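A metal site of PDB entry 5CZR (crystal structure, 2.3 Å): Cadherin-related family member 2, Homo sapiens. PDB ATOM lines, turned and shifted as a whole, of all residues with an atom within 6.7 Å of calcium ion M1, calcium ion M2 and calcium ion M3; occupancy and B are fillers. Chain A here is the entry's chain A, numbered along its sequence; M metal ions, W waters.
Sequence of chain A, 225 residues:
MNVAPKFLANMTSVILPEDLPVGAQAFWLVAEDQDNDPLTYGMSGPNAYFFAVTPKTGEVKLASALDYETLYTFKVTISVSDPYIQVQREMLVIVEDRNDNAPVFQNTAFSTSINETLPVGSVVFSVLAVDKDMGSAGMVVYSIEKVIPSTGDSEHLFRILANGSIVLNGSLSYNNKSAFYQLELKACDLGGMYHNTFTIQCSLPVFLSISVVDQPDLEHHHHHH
The side-chain hydroxyl (OG1) of Thr 70 lies within hydrogen-bond range of the side-chain carboxylate (OD2) of Asp 67, 3.2 Å away.
The side-chain amide nitrogen of Asn 101 lies close to the side-chain carboxylate of Glu 69 (3.4 Å).
The side-chain amide nitrogen (ND2) of Asn 101 lies close to the side-chain carboxylate (OD1) of Asp 100, at 2.8 Å.
The side-chain carboxylate (OE2) of Glu 18 lies close to the backbone NH (N) of Tyr 68 (3.0 Å).
The backbone NH (N) of Glu 18 sits at hydrogen-bond distance from the backbone carbonyl oxygen (O) of Glu 96 (3.0 Å).
O of Asn 99 is in hydrogen-bond range of NE2 of Gln 201 (2.8 Å).
The guanidinium group (NH2) of Arg 98 lies within salt-bridge range of the side-chain carboxylate (OE1) of Glu 96 (2.9 Å).
The side-chain carboxylate (OD1) of Asp 189 is in hydrogen-bond range of the backbone NH (N) of Gly 191, at 2.9 Å.
Four residues have an atom within 4 Å of calcium ion M1: Glu 18, Asp 67, Glu 69 and Asp 100.
Along chain A the residues within 4 Å of calcium ion M1 span positions 18 to 100.
The nearest printed residue that does not touch calcium ion M1 is Tyr 68 (4.1 Å).
Within 4 Å of calcium ion M3: Asn 99, Asn 101, Asp 131, Asp 133, Ala 137 and Asp 189.
Calcium ion M1 is bound by the side-chain carboxylate of Asp 67 (2.1 Å), water W1 (2.2 Å), water W2 (2.2 Å), the side-chain carboxylate of Glu 69 (2.2 Å), the side-chain carboxylate of Asp 100 (2.3 Å) and the side-chain carboxylate of Glu 18 (2.3 Å).
Calcium ion M2 is bound by the side-chain carboxylate (OD1) of Asp 97, at 2.2 Å.
Calcium ion M2 is bound by the side-chain carboxylate (OD1) of Asp 133, 2.3 Å away.
Calcium ion M2 is bound by the side-chain carboxylate (OD1) of Asp 100.
OE1 of Glu 18 is bound to calcium ion M2, 2.3 Å away.
Calcium ion M2 is bound by OE2 of Glu 69, at 2.4 Å.
Calcium ion M2 is bound by O of Arg 98, at 2.4 Å.
Calcium ion M2 has six donor atoms within binding distance.
Slightly farther from calcium ion M2 lies the side-chain carboxylate (OE1) of Glu 69 (2.9 Å).
Calcium ion M3 is bound by O of Asn 101 (2.2 Å).
OD1 of Asn 99 binds calcium ion M3 (2.3 Å).
Calcium ion M3 is bound by the backbone carbonyl oxygen (O) of Ala 137, at 2.3 Å.
OD2 of Asp 189 binds calcium ion M3 (2.5 Å).
OD2 of Asp 133 binds calcium ion M3.
OD2 of Asp 131 is bound to calcium ion M3 (2.5 Å).
Calcium ion M3 is bound by OD1 of Asp 131, 2.6 Å away.
Calcium ion M3 has seven donor atoms within binding distance.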
ATOM      1  N   GLU A  18      14.180 -21.114 -12.172  1.00  0.00           N
ATOM      2  CA  GLU A  18      13.174 -20.057 -12.069  1.00  0.00           C
ATOM      3  C   GLU A  18      11.817 -20.474 -12.678  1.00  0.00           C
ATOM      4  O   GLU A  18      10.804 -19.927 -12.297  1.00  0.00           O
ATOM      5  CB  GLU A  18      13.651 -18.725 -12.676  1.00  0.00           C
ATOM      6  CG  GLU A  18      13.899 -18.748 -14.183  1.00  0.00           C
ATOM      7  CD  GLU A  18      13.955 -17.368 -14.802  1.00  0.00           C
ATOM      8  OE1 GLU A  18      14.756 -17.180 -15.730  1.00  0.00           O
ATOM      9  OE2 GLU A  18      13.189 -16.480 -14.359  1.00  0.00           O
ATOM     10  N   LEU A  66       8.801 -18.365  -8.764  1.00  0.00           N
ATOM     11  CA  LEU A  66      10.138 -17.803  -8.785  1.00  0.00           C
ATOM     12  C   LEU A  66      10.325 -16.932 -10.012  1.00  0.00           C
ATOM     13  O   LEU A  66       9.585 -17.070 -10.981  1.00  0.00           O
ATOM     14  CB  LEU A  66      11.198 -18.920  -8.795  1.00  0.00           C
ATOM     15  CG  LEU A  66      11.093 -19.952  -7.649  1.00  0.00           C
ATOM     16  CD1 LEU A  66      12.123 -21.064  -7.819  1.00  0.00           C
ATOM     17  CD2 LEU A  66      11.303 -19.266  -6.294  1.00  0.00           C
ATOM     18  N   ASP A  67      11.338 -16.078  -9.994  1.00  0.00           N
ATOM     19  CA  ASP A  67      11.734 -15.306 -11.202  1.00  0.00           C
ATOM     20  C   ASP A  67      13.143 -14.767 -11.020  1.00  0.00           C
ATOM     21  O   ASP A  67      13.381 -13.946 -10.137  1.00  0.00           O
ATOM     22  CB  ASP A  67      10.739 -14.167 -11.468  1.00  0.00           C
ATOM     23  CG  ASP A  67      11.075 -13.342 -12.686  1.00  0.00           C
ATOM     24  OD1 ASP A  67      12.004 -13.709 -13.441  1.00  0.00           O
ATOM     25  OD2 ASP A  67      10.396 -12.311 -12.916  1.00  0.00           O
ATOM     26  N   TYR A  68      14.079 -15.297 -11.800  1.00  0.00           N
ATOM     27  CA  TYR A  68      15.489 -14.887 -11.739  1.00  0.00           C
ATOM     28  C   TYR A  68      15.625 -13.390 -11.985  1.00  0.00           C
ATOM     29  O   TYR A  68      16.479 -12.744 -11.388  1.00  0.00           O
ATOM     30  CB  TYR A  68      16.318 -15.651 -12.780  1.00  0.00           C
ATOM     31  CG  TYR A  68      17.784 -15.330 -12.735  1.00  0.00           C
ATOM     32  CD1 TYR A  68      18.666 -16.066 -11.915  1.00  0.00           C
ATOM     33  CD2 TYR A  68      18.306 -14.313 -13.511  1.00  0.00           C
ATOM     34  CE1 TYR A  68      20.028 -15.776 -11.854  1.00  0.00           C
ATOM     35  CE2 TYR A  68      19.671 -14.001 -13.468  1.00  0.00           C
ATOM     36  CZ  TYR A  68      20.523 -14.733 -12.648  1.00  0.00           C
ATOM     37  OH  TYR A  68      21.845 -14.407 -12.616  1.00  0.00           O
ATOM     38  N   GLU A  69      14.762 -12.835 -12.839  1.00  0.00           N
ATOM     39  CA  GLU A  69      14.876 -11.453 -13.239  1.00  0.00           C
ATOM     40  C   GLU A  69      14.440 -10.499 -12.110  1.00  0.00           C
ATOM     41  O   GLU A  69      14.673  -9.315 -12.202  1.00  0.00           O
ATOM     42  CB  GLU A  69      14.052 -11.194 -14.518  1.00  0.00           C
ATOM     43  CG  GLU A  69      14.732 -11.625 -15.826  1.00  0.00           C
ATOM     44  CD  GLU A  69      14.869 -13.124 -16.018  1.00  0.00           C
ATOM     45  OE1 GLU A  69      13.921 -13.865 -15.798  1.00  0.00           O
ATOM     46  OE2 GLU A  69      15.943 -13.609 -16.427  1.00  0.00           O
ATOM     47  N   THR A  70      13.823 -11.036 -11.062  1.00  0.00           N
ATOM     48  CA  THR A  70      13.201 -10.220  -9.992  1.00  0.00           C
ATOM     49  C   THR A  70      13.883 -10.439  -8.635  1.00  0.00           C
ATOM     50  O   THR A  70      14.075  -9.491  -7.897  1.00  0.00           O
ATOM     51  CB  THR A  70      11.718 -10.548  -9.945  1.00  0.00           C
ATOM     52  OG1 THR A  70      11.092  -9.849 -11.019  1.00  0.00           O
ATOM     53  CG2 THR A  70      11.028 -10.141  -8.647  1.00  0.00           C
ATOM     54  N   GLU A  96      18.120 -20.363 -10.490  1.00  0.00           N
ATOM     55  CA  GLU A  96      18.817 -20.438 -11.787  1.00  0.00           C
ATOM     56  C   GLU A  96      18.039 -19.772 -12.914  1.00  0.00           C
ATOM     57  O   GLU A  96      16.816 -19.910 -13.024  1.00  0.00           O
ATOM     58  CB  GLU A  96      19.096 -21.863 -12.176  1.00  0.00           C
ATOM     59  CG  GLU A  96      20.267 -22.458 -11.385  1.00  0.00           C
ATOM     60  CD  GLU A  96      20.894 -23.747 -11.963  1.00  0.00           C
ATOM     61  OE1 GLU A  96      20.225 -24.503 -12.687  1.00  0.00           O
ATOM     62  OE2 GLU A  96      22.059 -24.034 -11.636  1.00  0.00           O
ATOM     63  N   ASP A  97      18.764 -19.015 -13.730  1.00  0.00           N
ATOM     64  CA  ASP A  97      18.203 -18.363 -14.890  1.00  0.00           C
ATOM     65  C   ASP A  97      17.802 -19.414 -15.909  1.00  0.00           C
ATOM     66  O   ASP A  97      18.496 -20.386 -16.136  1.00  0.00           O
ATOM     67  CB  ASP A  97      19.208 -17.386 -15.482  1.00  0.00           C
ATOM     68  CG  ASP A  97      18.647 -16.589 -16.639  1.00  0.00           C
ATOM     69  OD1 ASP A  97      17.472 -16.122 -16.584  1.00  0.00           O
ATOM     70  OD2 ASP A  97      19.396 -16.433 -17.639  1.00  0.00           O
ATOM     71  N   ARG A  98      16.673 -19.177 -16.543  1.00  0.00           N
ATOM     72  CA  ARG A  98      16.255 -19.974 -17.666  1.00  0.00           C
ATOM     73  C   ARG A  98      15.936 -19.014 -18.820  1.00  0.00           C
ATOM     74  O   ARG A  98      15.837 -17.786 -18.623  1.00  0.00           O
ATOM     75  CB  ARG A  98      15.034 -20.818 -17.271  1.00  0.00           C
ATOM     76  CG  ARG A  98      15.315 -21.921 -16.228  1.00  0.00           C
ATOM     77  CD  ARG A  98      16.085 -23.048 -16.902  1.00  0.00           C
ATOM     78  NE  ARG A  98      16.644 -24.073 -16.040  1.00  0.00           N
ATOM     79  CZ  ARG A  98      17.870 -24.061 -15.547  1.00  0.00           C
ATOM     80  NH1 ARG A  98      18.708 -23.062 -15.774  1.00  0.00           N
ATOM     81  NH2 ARG A  98      18.241 -25.048 -14.793  1.00  0.00           N
ATOM     82  N   ASN A  99      15.762 -19.572 -20.026  1.00  0.00           N
ATOM     83  CA  ASN A  99      15.547 -18.717 -21.206  1.00  0.00           C
ATOM     84  C   ASN A  99      14.095 -18.309 -21.410  1.00  0.00           C
ATOM     85  O   ASN A  99      13.428 -18.783 -22.348  1.00  0.00           O
ATOM     86  CB  ASN A  99      16.107 -19.368 -22.457  1.00  0.00           C
ATOM     87  CG  ASN A  99      16.156 -18.415 -23.611  1.00  0.00           C
ATOM     88  OD1 ASN A  99      16.067 -17.215 -23.414  1.00  0.00           O
ATOM     89  ND2 ASN A  99      16.342 -18.942 -24.826  1.00  0.00           N
ATOM     90  N   ASP A 100      13.607 -17.434 -20.555  1.00  0.00           N
ATOM     91  CA  ASP A 100      12.196 -17.049 -20.527  1.00  0.00           C
ATOM     92  C   ASP A 100      11.916 -15.622 -21.032  1.00  0.00           C
ATOM     93  O   ASP A 100      10.774 -15.157 -20.963  1.00  0.00           O
ATOM     94  CB  ASP A 100      11.634 -17.199 -19.107  1.00  0.00           C
ATOM     95  CG  ASP A 100      12.325 -16.308 -18.099  1.00  0.00           C
ATOM     96  OD1 ASP A 100      13.415 -15.717 -18.388  1.00  0.00           O
ATOM     97  OD2 ASP A 100      11.764 -16.182 -16.995  1.00  0.00           O
ATOM     98  N   ASN A 101      12.945 -14.952 -21.553  1.00  0.00           N
ATOM     99  CA  ASN A 101      12.783 -13.683 -22.223  1.00  0.00           C
ATOM    100  C   ASN A 101      13.271 -13.725 -23.659  1.00  0.00           C
ATOM    101  O   ASN A 101      14.184 -14.487 -24.033  1.00  0.00           O
ATOM    102  CB  ASN A 101      13.546 -12.622 -21.461  1.00  0.00           C
ATOM    103  CG  ASN A 101      12.948 -12.321 -20.112  1.00  0.00           C
ATOM    104  OD1 ASN A 101      12.045 -11.517 -20.008  1.00  0.00           O
ATOM    105  ND2 ASN A 101      13.402 -13.024 -19.081  1.00  0.00           N
ATOM    106  N   ALA A 102      12.647 -12.888 -24.459  1.00  0.00           N
ATOM    107  CA  ALA A 102      12.967 -12.766 -25.872  1.00  0.00           C
ATOM    108  C   ALA A 102      13.708 -11.430 -26.072  1.00  0.00           C
ATOM    109  O   ALA A 102      13.533 -10.496 -25.304  1.00  0.00           O
ATOM    110  CB  ALA A 102      11.680 -12.768 -26.687  1.00  0.00           C
ATOM    111  N   PRO A 103      14.515 -11.321 -27.135  1.00  0.00           N
ATOM    112  CA  PRO A 103      15.010  -9.993 -27.453  1.00  0.00           C
ATOM    113  C   PRO A 103      13.893  -8.971 -27.773  1.00  0.00           C
ATOM    114  O   PRO A 103      12.905  -9.310 -28.411  1.00  0.00           O
ATOM    115  CB  PRO A 103      15.877 -10.243 -28.671  1.00  0.00           C
ATOM    116  CG  PRO A 103      16.246 -11.690 -28.597  1.00  0.00           C
ATOM    117  CD  PRO A 103      15.011 -12.345 -28.053  1.00  0.00           C
ATOM    118  N   ASP A 131      18.033  -8.567 -24.649  1.00  0.00           N
ATOM    119  CA  ASP A 131      17.431  -9.738 -24.015  1.00  0.00           C
ATOM    120  C   ASP A 131      17.925  -9.798 -22.585  1.00  0.00           C
ATOM    121  O   ASP A 131      19.126  -9.838 -22.338  1.00  0.00           O
ATOM    122  CB  ASP A 131      17.883 -10.970 -24.780  1.00  0.00           C
ATOM    123  CG  ASP A 131      17.165 -12.233 -24.365  1.00  0.00           C
ATOM    124  OD1 ASP A 131      17.232 -12.618 -23.178  1.00  0.00           O
ATOM    125  OD2 ASP A 131      16.623 -12.904 -25.261  1.00  0.00           O
ATOM    126  N   LYS A 132      17.003  -9.848 -21.637  1.00  0.00           N
ATOM    127  CA  LYS A 132      17.337  -9.844 -20.207  1.00  0.00           C
ATOM    128  C   LYS A 132      18.085 -11.059 -19.657  1.00  0.00           C
ATOM    129  O   LYS A 132      18.719 -10.970 -18.606  1.00  0.00           O
ATOM    130  CB  LYS A 132      16.054  -9.737 -19.389  1.00  0.00           C
ATOM    131  CG  LYS A 132      15.349  -8.401 -19.542  1.00  0.00           C
ATOM    132  CD  LYS A 132      13.913  -8.518 -19.062  1.00  0.00           C
ATOM    133  CE  LYS A 132      13.172  -7.198 -19.241  1.00  0.00           C
ATOM    134  NZ  LYS A 132      11.949  -7.236 -18.406  1.00  0.00           N
ATOM    135  N   ASP A 133      17.996 -12.187 -20.334  1.00  0.00           N
ATOM    136  CA  ASP A 133      18.552 -13.417 -19.799  1.00  0.00           C
ATOM    137  C   ASP A 133      20.072 -13.367 -19.782  1.00  0.00           C
ATOM    138  O   ASP A 133      20.662 -12.491 -20.381  1.00  0.00           O
ATOM    139  CB  ASP A 133      18.036 -14.624 -20.585  1.00  0.00           C
ATOM    140  CG  ASP A 133      16.517 -14.781 -20.461  1.00  0.00           C
ATOM    141  OD1 ASP A 133      15.990 -14.686 -19.334  1.00  0.00           O
ATOM    142  OD2 ASP A 133      15.841 -14.971 -21.486  1.00  0.00           O
ATOM    143  N   MET A 134      20.681 -14.277 -19.009  1.00  0.00           N
ATOM    144  CA  MET A 134      22.134 -14.405 -18.871  1.00  0.00           C
ATOM    145  C   MET A 134      22.734 -15.337 -19.934  1.00  0.00           C
ATOM    146  O   MET A 134      22.065 -16.187 -20.489  1.00  0.00           O
ATOM    147  CB  MET A 134      22.474 -14.953 -17.471  1.00  0.00           C
ATOM    148  CG  MET A 134      22.031 -14.055 -16.300  1.00  0.00           C
ATOM    149  SD  MET A 134      22.828 -12.428 -16.370  1.00  0.00           S
ATOM    150  CE  MET A 134      22.208 -11.701 -14.868  1.00  0.00           C
ATOM    151  N   SER A 136      24.237 -17.276 -23.041  1.00  0.00           N
ATOM    152  CA  SER A 136      23.810 -17.423 -24.428  1.00  0.00           C
ATOM    153  C   SER A 136      22.347 -17.077 -24.573  1.00  0.00           C
ATOM    154  O   SER A 136      21.910 -16.619 -25.640  1.00  0.00           O
ATOM    155  CB  SER A 136      23.981 -18.850 -24.906  1.00  0.00           C
ATOM    156  OG  SER A 136      25.345 -19.174 -24.839  1.00  0.00           O
ATOM    157  N   ALA A 137      21.584 -17.315 -23.497  1.00  0.00           N
ATOM    158  CA  ALA A 137      20.160 -17.017 -23.524  1.00  0.00           C
ATOM    159  C   ALA A 137      19.853 -15.522 -23.654  1.00  0.00           C
ATOM    160  O   ALA A 137      18.697 -15.157 -23.961  1.00  0.00           O
ATOM    161  CB  ALA A 137      19.500 -17.610 -22.298  1.00  0.00           C
ATOM    162  N   GLY A 138      20.862 -14.683 -23.399  1.00  0.00           N
ATOM    163  CA  GLY A 138      20.786 -13.255 -23.569  1.00  0.00           C
ATOM    164  C   GLY A 138      21.598 -12.658 -24.732  1.00  0.00           C
ATOM    165  O   GLY A 138      21.559 -11.443 -24.916  1.00  0.00           O
ATOM    166  N   MET A 139      22.332 -13.497 -25.478  1.00  0.00           N
ATOM    167  CA  MET A 139      23.112 -13.025 -26.643  1.00  0.00           C
ATOM    168  C   MET A 139      22.191 -12.924 -27.841  1.00  0.00           C
ATOM    169  O   MET A 139      21.493 -13.857 -28.205  1.00  0.00           O
ATOM    170  CB  MET A 139      24.306 -13.936 -26.947  1.00  0.00           C
ATOM    171  CG  MET A 139      25.457 -13.850 -25.927  1.00  0.00           C
ATOM    172  SD  MET A 139      26.891 -14.945 -26.212  1.00  0.00           S
ATOM    173  CE  MET A 139      27.776 -14.995 -24.628  1.00  0.00           C
ATOM    174  N   ASP A 189      17.780 -14.996 -29.482  1.00  0.00           N
ATOM    175  CA  ASP A 189      18.906 -15.321 -28.591  1.00  0.00           C
ATOM    176  C   ASP A 189      19.585 -16.546 -29.137  1.00  0.00           C
ATOM    177  O   ASP A 189      19.119 -17.110 -30.106  1.00  0.00           O
ATOM    178  CB  ASP A 189      18.509 -15.449 -27.106  1.00  0.00           C
ATOM    179  CG  ASP A 189      17.398 -16.449 -26.852  1.00  0.00           C
ATOM    180  OD1 ASP A 189      17.405 -17.565 -27.451  1.00  0.00           O
ATOM    181  OD2 ASP A 189      16.498 -16.158 -26.040  1.00  0.00           O
ATOM    182  N   LEU A 190      20.688 -16.971 -28.533  1.00  0.00           N
ATOM    183  CA  LEU A 190      21.375 -18.220 -28.910  1.00  0.00           C
ATOM    184  C   LEU A 190      20.888 -19.415 -28.150  1.00  0.00           C
ATOM    185  O   LEU A 190      21.427 -20.507 -28.253  1.00  0.00           O
ATOM    186  CB  LEU A 190      22.890 -18.078 -28.716  1.00  0.00           C
ATOM    187  CG  LEU A 190      23.537 -17.107 -29.719  1.00  0.00           C
ATOM    188  CD1 LEU A 190      24.988 -16.866 -29.348  1.00  0.00           C
ATOM    189  CD2 LEU A 190      23.399 -17.636 -31.150  1.00  0.00           C
ATOM    190  N   GLY A 191      19.831 -19.218 -27.356  1.00  0.00           N
ATOM    191  CA  GLY A 191      19.151 -20.342 -26.720  1.00  0.00           C
ATOM    192  C   GLY A 191      19.652 -20.699 -25.326  1.00  0.00           C
ATOM    193  O   GLY A 191      20.683 -20.187 -24.852  1.00  0.00           O
ATOM    194  N   GLN A 201      14.525 -18.057 -28.192  1.00  0.00           N
ATOM    195  CA  GLN A 201      13.487 -17.003 -28.191  1.00  0.00           C
ATOM    196  C   GLN A 201      13.769 -15.962 -29.229  1.00  0.00           C
ATOM    197  O   GLN A 201      14.917 -15.568 -29.392  1.00  0.00           O
ATOM    198  CB  GLN A 201      13.384 -16.304 -26.820  1.00  0.00           C
ATOM    199  CG  GLN A 201      13.195 -17.242 -25.646  1.00  0.00           C
ATOM    200  CD  GLN A 201      11.730 -17.597 -25.411  1.00  0.00           C
ATOM    201  OE1 GLN A 201      10.869 -17.324 -26.235  1.00  0.00           O
ATOM    202  NE2 GLN A 201      11.441 -18.203 -24.274  1.00  0.00           N
HETATM  203 CA    CA M   1      11.969 -14.781 -15.235  1.00  0.00          CA
HETATM  204 CA    CA M   2      15.506 -15.737 -17.385  1.00  0.00          CA
HETATM  205 CA    CA M   3      16.367 -14.961 -23.897  1.00  0.00          CA
HETATM  206  O   HOH W   1      11.262 -13.354 -16.714  1.00  0.00           O
HETATM  207  O   HOH W   2      10.026 -15.638 -14.585  1.00  0.00           O
